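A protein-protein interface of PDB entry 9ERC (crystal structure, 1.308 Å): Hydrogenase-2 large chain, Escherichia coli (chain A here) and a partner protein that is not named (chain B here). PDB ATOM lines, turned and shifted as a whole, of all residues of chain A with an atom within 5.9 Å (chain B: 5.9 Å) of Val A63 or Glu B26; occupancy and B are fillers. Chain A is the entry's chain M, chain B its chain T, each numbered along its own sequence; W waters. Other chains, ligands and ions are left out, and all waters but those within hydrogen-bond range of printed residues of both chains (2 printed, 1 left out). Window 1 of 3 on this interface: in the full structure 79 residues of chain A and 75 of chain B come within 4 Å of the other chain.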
ATOM      1  N   GLU A  14     -13.802 -24.520 -27.263  1.00  0.00           N
ATOM      2  CA  GLU A  14     -14.135 -25.386 -26.148  1.00  0.00           C
ATOM      3  C   GLU A  14     -14.585 -26.746 -26.695  1.00  0.00           C
ATOM      4  O   GLU A  14     -15.464 -26.823 -27.554  1.00  0.00           O
ATOM      5  CB  GLU A  14     -15.243 -24.761 -25.301  1.00  0.00           C
ATOM      6  CG  GLU A  14     -15.461 -25.477 -23.968  1.00  0.00           C
ATOM      7  CD  GLU A  14     -16.008 -26.895 -24.084  1.00  0.00           C
ATOM      8  OE1 GLU A  14     -16.837 -27.098 -25.006  1.00  0.00           O
ATOM      9  OE2 GLU A  14     -15.597 -27.811 -23.293  1.00  0.00           O
ATOM     10  N   CYS A  61     -20.941 -26.528 -19.266  1.00  0.00           N
ATOM     11  CA  CYS A  61     -19.795 -25.811 -19.819  1.00  0.00           C
ATOM     12  C   CYS A  61     -19.155 -24.859 -18.816  1.00  0.00           C
ATOM     13  O   CYS A  61     -19.857 -24.154 -18.104  1.00  0.00           O
ATOM     14  CB  CYS A  61     -20.214 -25.067 -21.065  1.00  0.00           C
ATOM     15  SG  CYS A  61     -18.845 -24.285 -21.953  1.00  0.00           S
ATOM     16  N   GLY A  62     -17.821 -24.865 -18.794  1.00  0.00           N
ATOM     17  CA  GLY A  62     -17.066 -23.999 -17.901  1.00  0.00           C
ATOM     18  C   GLY A  62     -16.494 -22.783 -18.608  1.00  0.00           C
ATOM     19  O   GLY A  62     -15.958 -21.901 -17.939  1.00  0.00           O
ATOM     20  N   VAL A  63     -16.536 -22.771 -19.950  1.00  0.00           N
ATOM     21  CA  VAL A  63     -16.191 -21.578 -20.690  1.00  0.00           C
ATOM     22  C   VAL A  63     -17.355 -20.608 -20.581  1.00  0.00           C
ATOM     23  O   VAL A  63     -17.216 -19.554 -20.002  1.00  0.00           O
ATOM     24  CB  VAL A  63     -15.844 -21.904 -22.159  1.00  0.00           C
ATOM     25  CG1 VAL A  63     -15.699 -20.662 -22.993  1.00  0.00           C
ATOM     26  CG2 VAL A  63     -14.587 -22.768 -22.223  1.00  0.00           C
ATOM     27  N   CYS A  64     -18.545 -21.052 -20.996  1.00  0.00           N
ATOM     28  CA  CYS A  64     -19.760 -20.295 -20.757  1.00  0.00           C
ATOM     29  C   CYS A  64     -20.363 -20.698 -19.420  1.00  0.00           C
ATOM     30  O   CYS A  64     -21.546 -21.007 -19.282  1.00  0.00           O
ATOM     31  CB  CYS A  64     -20.740 -20.352 -21.908  1.00  0.00           C
ATOM     32  SG  CYS A  64     -21.422 -21.995 -22.217  1.00  0.00           S
ATOM     33  N   THR A  65     -19.511 -20.641 -18.394  1.00  0.00           N
ATOM     34  CA  THR A  65     -20.002 -20.777 -17.033  1.00  0.00           C
ATOM     35  C   THR A  65     -21.023 -19.663 -16.806  1.00  0.00           C
ATOM     36  O   THR A  65     -21.058 -18.703 -17.566  1.00  0.00           O
ATOM     37  CB  THR A  65     -18.820 -20.846 -16.046  1.00  0.00           C
ATOM     38  OG1 THR A  65     -19.343 -21.199 -14.772  1.00  0.00           O
ATOM     39  CG2 THR A  65     -18.085 -19.538 -15.918  1.00  0.00           C
ATOM     40  N   HIS A  99     -19.370 -11.906 -17.068  1.00  0.00           N
ATOM     41  CA  HIS A  99     -18.887 -13.169 -17.593  1.00  0.00           C
ATOM     42  C   HIS A  99     -18.679 -13.034 -19.109  1.00  0.00           C
ATOM     43  O   HIS A  99     -17.656 -13.444 -19.636  1.00  0.00           O
ATOM     44  CB  HIS A  99     -19.905 -14.305 -17.372  1.00  0.00           C
ATOM     45  CG  HIS A  99     -19.451 -15.464 -18.141  1.00  0.00           C
ATOM     46  ND1 HIS A  99     -18.405 -16.263 -17.741  1.00  0.00           N
ATOM     47  CD2 HIS A  99     -19.761 -15.823 -19.411  1.00  0.00           C
ATOM     48  CE1 HIS A  99     -18.112 -17.093 -18.747  1.00  0.00           C
ATOM     49  NE2 HIS A  99     -18.918 -16.833 -19.769  1.00  0.00           N
ATOM     50  N   HIS A 102     -15.529 -11.273 -20.210  1.00  0.00           N
ATOM     51  CA  HIS A 102     -14.395 -12.200 -20.144  1.00  0.00           C
ATOM     52  C   HIS A 102     -14.401 -13.131 -21.358  1.00  0.00           C
ATOM     53  O   HIS A 102     -13.369 -13.367 -21.991  1.00  0.00           O
ATOM     54  CB  HIS A 102     -14.442 -12.981 -18.826  1.00  0.00           C
ATOM     55  CG  HIS A 102     -14.014 -14.386 -18.940  1.00  0.00           C
ATOM     56  ND1 HIS A 102     -12.712 -14.843 -18.862  1.00  0.00           N
ATOM     57  CD2 HIS A 102     -14.786 -15.482 -19.103  1.00  0.00           C
ATOM     58  CE1 HIS A 102     -12.729 -16.175 -19.021  1.00  0.00           C
ATOM     59  NE2 HIS A 102     -13.972 -16.578 -19.191  1.00  0.00           N
ATOM     60  N   ASP A 103     -15.573 -13.683 -21.637  1.00  0.00           N
ATOM     61  CA  ASP A 103     -15.706 -14.746 -22.613  1.00  0.00           C
ATOM     62  C   ASP A 103     -15.307 -14.207 -23.992  1.00  0.00           C
ATOM     63  O   ASP A 103     -14.499 -14.795 -24.691  1.00  0.00           O
ATOM     64  CB  ASP A 103     -17.156 -15.261 -22.530  1.00  0.00           C
ATOM     65  CG  ASP A 103     -17.375 -16.642 -23.114  1.00  0.00           C
ATOM     66  OD1 ASP A 103     -16.674 -16.951 -24.105  1.00  0.00           O
ATOM     67  OD2 ASP A 103     -18.269 -17.389 -22.612  1.00  0.00           O
ATOM     68  N   VAL A 106     -11.525 -13.353 -24.417  1.00  0.00           N
ATOM     69  CA  VAL A 106     -10.716 -14.550 -24.526  1.00  0.00           C
ATOM     70  C   VAL A 106     -10.911 -15.161 -25.918  1.00  0.00           C
ATOM     71  O   VAL A 106      -9.954 -15.667 -26.526  1.00  0.00           O
ATOM     72  CB  VAL A 106     -11.046 -15.511 -23.378  1.00  0.00           C
ATOM     73  CG1 VAL A 106     -10.434 -16.878 -23.583  1.00  0.00           C
ATOM     74  CG2 VAL A 106     -10.577 -14.914 -22.048  1.00  0.00           C
ATOM     75  N   LEU A 111      -8.388 -17.502 -28.262  1.00  0.00           N
ATOM     76  CA  LEU A 111      -8.876 -18.558 -29.128  1.00  0.00           C
ATOM     77  C   LEU A 111      -8.683 -18.216 -30.609  1.00  0.00           C
ATOM     78  O   LEU A 111      -8.374 -19.130 -31.366  1.00  0.00           O
ATOM     79  CB  LEU A 111     -10.336 -18.876 -28.801  1.00  0.00           C
ATOM     80  CG  LEU A 111     -10.599 -19.244 -27.341  1.00  0.00           C
ATOM     81  CD1 LEU A 111     -12.069 -19.554 -27.107  1.00  0.00           C
ATOM     82  CD2 LEU A 111      -9.725 -20.404 -26.878  1.00  0.00           C
ATOM     83  N   GLN A 198      -9.696  -9.631 -18.918  1.00  0.00           N
ATOM     84  CA  GLN A 198     -10.631 -10.714 -18.629  1.00  0.00           C
ATOM     85  C   GLN A 198     -10.565 -11.136 -17.159  1.00  0.00           C
ATOM     86  O   GLN A 198     -11.593 -11.556 -16.611  1.00  0.00           O
ATOM     87  CB  GLN A 198     -10.455 -11.870 -19.614  1.00  0.00           C
ATOM     88  CG  GLN A 198      -9.151 -12.652 -19.486  1.00  0.00           C
ATOM     89  CD  GLN A 198      -9.118 -13.684 -18.378  1.00  0.00           C
ATOM     90  OE1 GLN A 198     -10.127 -14.300 -18.020  1.00  0.00           O
ATOM     91  NE2 GLN A 198      -7.942 -13.908 -17.820  1.00  0.00           N
ATOM     92  N   ASN A 202     -13.802 -11.265 -14.464  1.00  0.00           N
ATOM     93  CA  ASN A 202     -14.172 -12.409 -13.652  1.00  0.00           C
ATOM     94  C   ASN A 202     -14.105 -12.084 -12.161  1.00  0.00           C
ATOM     95  O   ASN A 202     -14.695 -12.803 -11.370  1.00  0.00           O
ATOM     96  CB  ASN A 202     -13.381 -13.648 -14.000  1.00  0.00           C
ATOM     97  CG  ASN A 202     -14.080 -14.367 -15.142  1.00  0.00           C
ATOM     98  OD1 ASN A 202     -15.297 -14.237 -15.350  1.00  0.00           O
ATOM     99  ND2 ASN A 202     -13.303 -15.114 -15.866  1.00  0.00           N
ATOM    100  N   PRO A 213     -14.506 -20.251 -12.280  1.00  0.00           N
ATOM    101  CA  PRO A 213     -15.710 -20.830 -12.875  1.00  0.00           C
ATOM    102  C   PRO A 213     -16.694 -21.467 -11.898  1.00  0.00           C
ATOM    103  O   PRO A 213     -16.347 -21.887 -10.798  1.00  0.00           O
ATOM    104  CB  PRO A 213     -15.162 -21.956 -13.784  1.00  0.00           C
ATOM    105  CG  PRO A 213     -13.732 -21.565 -14.015  1.00  0.00           C
ATOM    106  CD  PRO A 213     -13.285 -20.943 -12.707  1.00  0.00           C
ATOM    107  N   ARG A 479     -22.578 -17.149 -27.022  1.00  0.00           N
ATOM    108  CA  ARG A 479     -22.608 -17.810 -28.324  1.00  0.00           C
ATOM    109  C   ARG A 479     -24.006 -17.832 -28.936  1.00  0.00           C
ATOM    110  O   ARG A 479     -24.161 -18.319 -30.058  1.00  0.00           O
ATOM    111  CB  ARG A 479     -22.053 -19.218 -28.158  1.00  0.00           C
ATOM    112  CG  ARG A 479     -20.551 -19.184 -27.894  1.00  0.00           C
ATOM    113  CD  ARG A 479     -19.940 -20.456 -27.353  1.00  0.00           C
ATOM    114  NE  ARG A 479     -18.545 -20.255 -26.984  1.00  0.00           N
ATOM    115  CZ  ARG A 479     -18.141 -19.565 -25.930  1.00  0.00           C
ATOM    116  NH1 ARG A 479     -18.969 -19.239 -24.976  1.00  0.00           N
ATOM    117  NH2 ARG A 479     -16.864 -19.256 -25.798  1.00  0.00           N
ATOM    118  N   ASP A 544     -17.244 -19.187 -32.580  1.00  0.00           N
ATOM    119  CA  ASP A 544     -16.922 -19.425 -31.173  1.00  0.00           C
ATOM    120  C   ASP A 544     -17.467 -20.778 -30.731  1.00  0.00           C
ATOM    121  O   ASP A 544     -18.236 -20.896 -29.767  1.00  0.00           O
ATOM    122  CB  ASP A 544     -17.411 -18.237 -30.362  1.00  0.00           C
ATOM    123  CG  ASP A 544     -16.992 -18.201 -28.904  1.00  0.00           C
ATOM    124  OD1 ASP A 544     -16.156 -19.041 -28.468  1.00  0.00           O
ATOM    125  OD2 ASP A 544     -17.558 -17.340 -28.219  1.00  0.00           O
ATOM    126  N   CYS A 546     -18.453 -24.177 -29.025  1.00  0.00           N
ATOM    127  CA  CYS A 546     -18.377 -24.734 -27.696  1.00  0.00           C
ATOM    128  C   CYS A 546     -19.083 -26.079 -27.747  1.00  0.00           C
ATOM    129  O   CYS A 546     -20.307 -26.125 -27.815  1.00  0.00           O
ATOM    130  CB  CYS A 546     -18.989 -23.770 -26.708  1.00  0.00           C
ATOM    131  SG  CYS A 546     -18.811 -24.339 -25.009  1.00  0.00           S
ATOM    132  N   CYS B  21     -15.662 -30.012 -19.152  1.00  0.00           N
ATOM    133  CA  CYS B  21     -16.478 -28.849 -19.479  1.00  0.00           C
ATOM    134  C   CYS B  21     -15.598 -27.627 -19.785  1.00  0.00           C
ATOM    135  O   CYS B  21     -16.112 -26.587 -20.196  1.00  0.00           O
ATOM    136  CB  CYS B  21     -17.472 -28.527 -18.368  1.00  0.00           C
ATOM    137  SG  CYS B  21     -16.731 -27.643 -16.962  1.00  0.00           S
ATOM    138  N   THR B  22     -14.290 -27.776 -19.550  1.00  0.00           N
ATOM    139  CA  THR B  22     -13.248 -26.773 -19.775  1.00  0.00           C
ATOM    140  C   THR B  22     -13.098 -25.854 -18.566  1.00  0.00           C
ATOM    141  O   THR B  22     -12.178 -25.046 -18.529  1.00  0.00           O
ATOM    142  CB  THR B  22     -13.371 -26.059 -21.124  1.00  0.00           C
ATOM    143  OG1 THR B  22     -13.549 -27.080 -22.117  1.00  0.00           O
ATOM    144  CG2 THR B  22     -12.169 -25.204 -21.455  1.00  0.00           C
ATOM    145  N   GLY B  23     -13.928 -26.041 -17.545  1.00  0.00           N
ATOM    146  CA  GLY B  23     -13.836 -25.238 -16.326  1.00  0.00           C
ATOM    147  C   GLY B  23     -12.498 -25.369 -15.610  1.00  0.00           C
ATOM    148  O   GLY B  23     -12.022 -24.413 -14.993  1.00  0.00           O
ATOM    149  N   CYS B  24     -11.899 -26.558 -15.668  1.00  0.00           N
ATOM    150  CA  CYS B  24     -10.605 -26.778 -15.034  1.00  0.00           C
ATOM    151  C   CYS B  24      -9.490 -26.006 -15.734  1.00  0.00           C
ATOM    152  O   CYS B  24      -8.672 -25.394 -15.065  1.00  0.00           O
ATOM    153  CB  CYS B  24     -10.310 -28.266 -14.892  1.00  0.00           C
ATOM    154  SG  CYS B  24     -11.368 -29.086 -13.672  1.00  0.00           S
ATOM    155  N   THR B  25      -9.484 -25.952 -17.072  1.00  0.00           N
ATOM    156  CA  THR B  25      -8.571 -25.070 -17.793  1.00  0.00           C
ATOM    157  C   THR B  25      -8.882 -23.609 -17.479  1.00  0.00           C
ATOM    158  O   THR B  25      -7.981 -22.791 -17.231  1.00  0.00           O
ATOM    159  CB  THR B  25      -8.652 -25.315 -19.304  1.00  0.00           C
ATOM    160  OG1 THR B  25      -8.065 -26.603 -19.543  1.00  0.00           O
ATOM    161  CG2 THR B  25      -7.948 -24.238 -20.101  1.00  0.00           C
ATOM    162  N   GLU B  26     -10.182 -23.273 -17.489  1.00  0.00           N
ATOM    163  CA  GLU B  26     -10.584 -21.889 -17.271  1.00  0.00           C
ATOM    164  C   GLU B  26     -10.161 -21.389 -15.888  1.00  0.00           C
ATOM    165  O   GLU B  26      -9.916 -20.196 -15.727  1.00  0.00           O
ATOM    166  CB  GLU B  26     -12.101 -21.758 -17.407  1.00  0.00           C
ATOM    167  CG  GLU B  26     -12.541 -21.726 -18.850  1.00  0.00           C
ATOM    168  CD  GLU B  26     -12.330 -20.400 -19.564  1.00  0.00           C
ATOM    169  OE1 GLU B  26     -11.805 -19.452 -18.962  1.00  0.00           O
ATOM    170  OE2 GLU B  26     -12.651 -20.316 -20.766  1.00  0.00           O
ATOM    171  N   SER B  27     -10.052 -22.285 -14.913  1.00  0.00           N
ATOM    172  CA  SER B  27      -9.557 -21.872 -13.594  1.00  0.00           C
ATOM    173  C   SER B  27      -8.222 -21.150 -13.738  1.00  0.00           C
ATOM    174  O   SER B  27      -7.919 -20.170 -13.029  1.00  0.00           O
ATOM    175  CB  SER B  27      -9.498 -23.001 -12.617  1.00  0.00           C
ATOM    176  OG  SER B  27      -8.381 -23.875 -12.822  1.00  0.00           O
ATOM    177  N   LEU B  28      -7.381 -21.623 -14.662  1.00  0.00           N
ATOM    178  CA  LEU B  28      -6.051 -21.032 -14.827  1.00  0.00           C
ATOM    179  C   LEU B  28      -6.116 -19.561 -15.198  1.00  0.00           C
ATOM    180  O   LEU B  28      -5.168 -18.831 -14.921  1.00  0.00           O
ATOM    181  CB  LEU B  28      -5.266 -21.765 -15.917  1.00  0.00           C
ATOM    182  CG  LEU B  28      -5.029 -23.248 -15.670  1.00  0.00           C
ATOM    183  CD1 LEU B  28      -4.229 -23.853 -16.814  1.00  0.00           C
ATOM    184  CD2 LEU B  28      -4.296 -23.467 -14.366  1.00  0.00           C
ATOM    185  N   LEU B  29      -7.195 -19.131 -15.864  1.00  0.00           N
ATOM    186  CA  LEU B  29      -7.348 -17.763 -16.333  1.00  0.00           C
ATOM    187  C   LEU B  29      -7.706 -16.843 -15.180  1.00  0.00           C
ATOM    188  O   LEU B  29      -7.640 -15.645 -15.384  1.00  0.00           O
ATOM    189  CB  LEU B  29      -8.376 -17.652 -17.464  1.00  0.00           C
ATOM    190  CG  LEU B  29      -7.791 -17.828 -18.869  1.00  0.00           C
ATOM    191  CD1 LEU B  29      -7.160 -19.200 -19.060  1.00  0.00           C
ATOM    192  CD2 LEU B  29      -8.844 -17.570 -19.895  1.00  0.00           C
ATOM    193  N   ARG B  30      -8.041 -17.399 -14.009  1.00  0.00           N
ATOM    194  CA  ARG B  30      -8.264 -16.605 -12.802  1.00  0.00           C
ATOM    195  C   ARG B  30      -7.011 -16.542 -11.930  1.00  0.00           C
ATOM    196  O   ARG B  30      -6.951 -15.711 -11.017  1.00  0.00           O
ATOM    197  CB  ARG B  30      -9.398 -17.176 -11.953  1.00  0.00           C
ATOM    198  CG  ARG B  30     -10.792 -16.973 -12.521  1.00  0.00           C
ATOM    199  CD  ARG B  30     -11.071 -17.842 -13.745  1.00  0.00           C
ATOM    200  NE  ARG B  30     -12.499 -17.888 -14.052  1.00  0.00           N
ATOM    201  CZ  ARG B  30     -12.999 -18.157 -15.252  1.00  0.00           C
ATOM    202  NH1 ARG B  30     -12.195 -18.418 -16.265  1.00  0.00           N
ATOM    203  NH2 ARG B  30     -14.309 -18.206 -15.434  1.00  0.00           N
HETATM  204  O   HOH W   1     -10.644 -14.969 -15.298  1.00  0.00           O
HETATM  205  O   HOH W   2     -13.010 -17.991 -21.685  1.00  0.00           O
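Printed residues of chain B within 4 Å of Gly A62: Cys B21, Gly B23 and Glu B26.
Val A63 touches just these residues of chain B: Cys B21 (3.8 Å), Thr B22 (3.5 Å) and Glu B26 (3.4 Å).
Of the printed residues of chain B, Gln A198 touches Leu B29 (3.0 Å).
Asp A544 touches none of the printed residues of chain B.
Cys A546 touches none of the printed residues of chain B.
Of chain A, only Gly A62, Val A63, His A102 and Pro A213 come within 4 Å of Glu B26.
The nearest residue of chain B that does not touch Val A63 is Gly B23 (4.8 Å).
The nearest residue of chain A that does not touch Glu B26 is Val A106 (5.0 Å).
O of Cys B21 is in hydrogen-bond range of N of Gly A62 (2.8 Å).
The side-chain carboxylate (OE2) of Glu A14 sits close to the backbone carbonyl oxygen (O) of Cys B21 (3.4 Å).
The side-chain hydroxyl of Thr B22 sits at hydrogen-bond distance from the side-chain carboxylate of Glu A14 (2.5 Å).
The side-chain amide nitrogen (NE2) of Gln A198 sits at hydrogen-bond distance from the backbone carbonyl oxygen (O) of Leu B29 (3.0 Å).
NH2 of Arg B30 sits close to ND2 of Asn A202.
Among the printed residues, merely in contact across the chains: His A102 with Glu B26 (3.4 Å), Pro A213 with Arg B30 (3.4 Å), Val A63 with Glu B26 (3.4 Å), Pro A213 with Gly B23 (3.5 Å), Val A63 with Thr B22 (3.5 Å), Gly A62 with Glu B26 (3.5 Å), His A102 with Arg B30 (3.6 Å), Gly A62 with Gly B23 (3.8 Å), Cys A61 with Cys B21 (3.8 Å), Pro A213 with Glu B26 (3.8 Å), Val A106 with Leu B29 (3.8 Å), Val A63 with Cys B21 (3.8 Å) and Pro A213 with Ser B27 (3.9 Å).
Printed residues of chain B that touch a printed residue of chain A: Cys B21, Thr B22, Gly B23, Glu B26, Ser B27, Leu B29 and Arg B30.
Hydrophobic or aromatic side chains of chain B that line the printed part of chain A: Leu B29.
Among the printed residues, no Asp or Glu carboxylate lies within 4 Å of a Lys or Arg side-chain nitrogen of the other chain.
OE1 of Glu A14 sits close to SG of Cys A546 (3.4 Å).
OE1 of Glu B26 is in salt-bridge range of NH1 of Arg B30, at 2.9 Å.
A ring nitrogen (ND1) of His A102 lies within hydrogen-bond range of the side-chain amide oxygen of Gln A198, at 2.8 Å.
The backbone carbonyl oxygen (O) of Val A106 sits at hydrogen-bond distance from the backbone NH (N) of Leu A111.
The backbone NH (N) of Val A63 sits close to the side-chain sulfur (SG) of Cys A61 (3.4 Å).
ND1 of His A102 lies within hydrogen-bond range of ND2 of Asn A202 (3.1 Å).
Water W2 lies within hydrogen-bond range of the side-chain carboxylate of Glu B26 (2.5 Å) and a ring nitrogen (NE2) of His A102 (3.0 Å).
Water W1 lies within hydrogen-bond range of ND2 of Asn A202, OE1 of Gln A198 and O of Leu B29.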
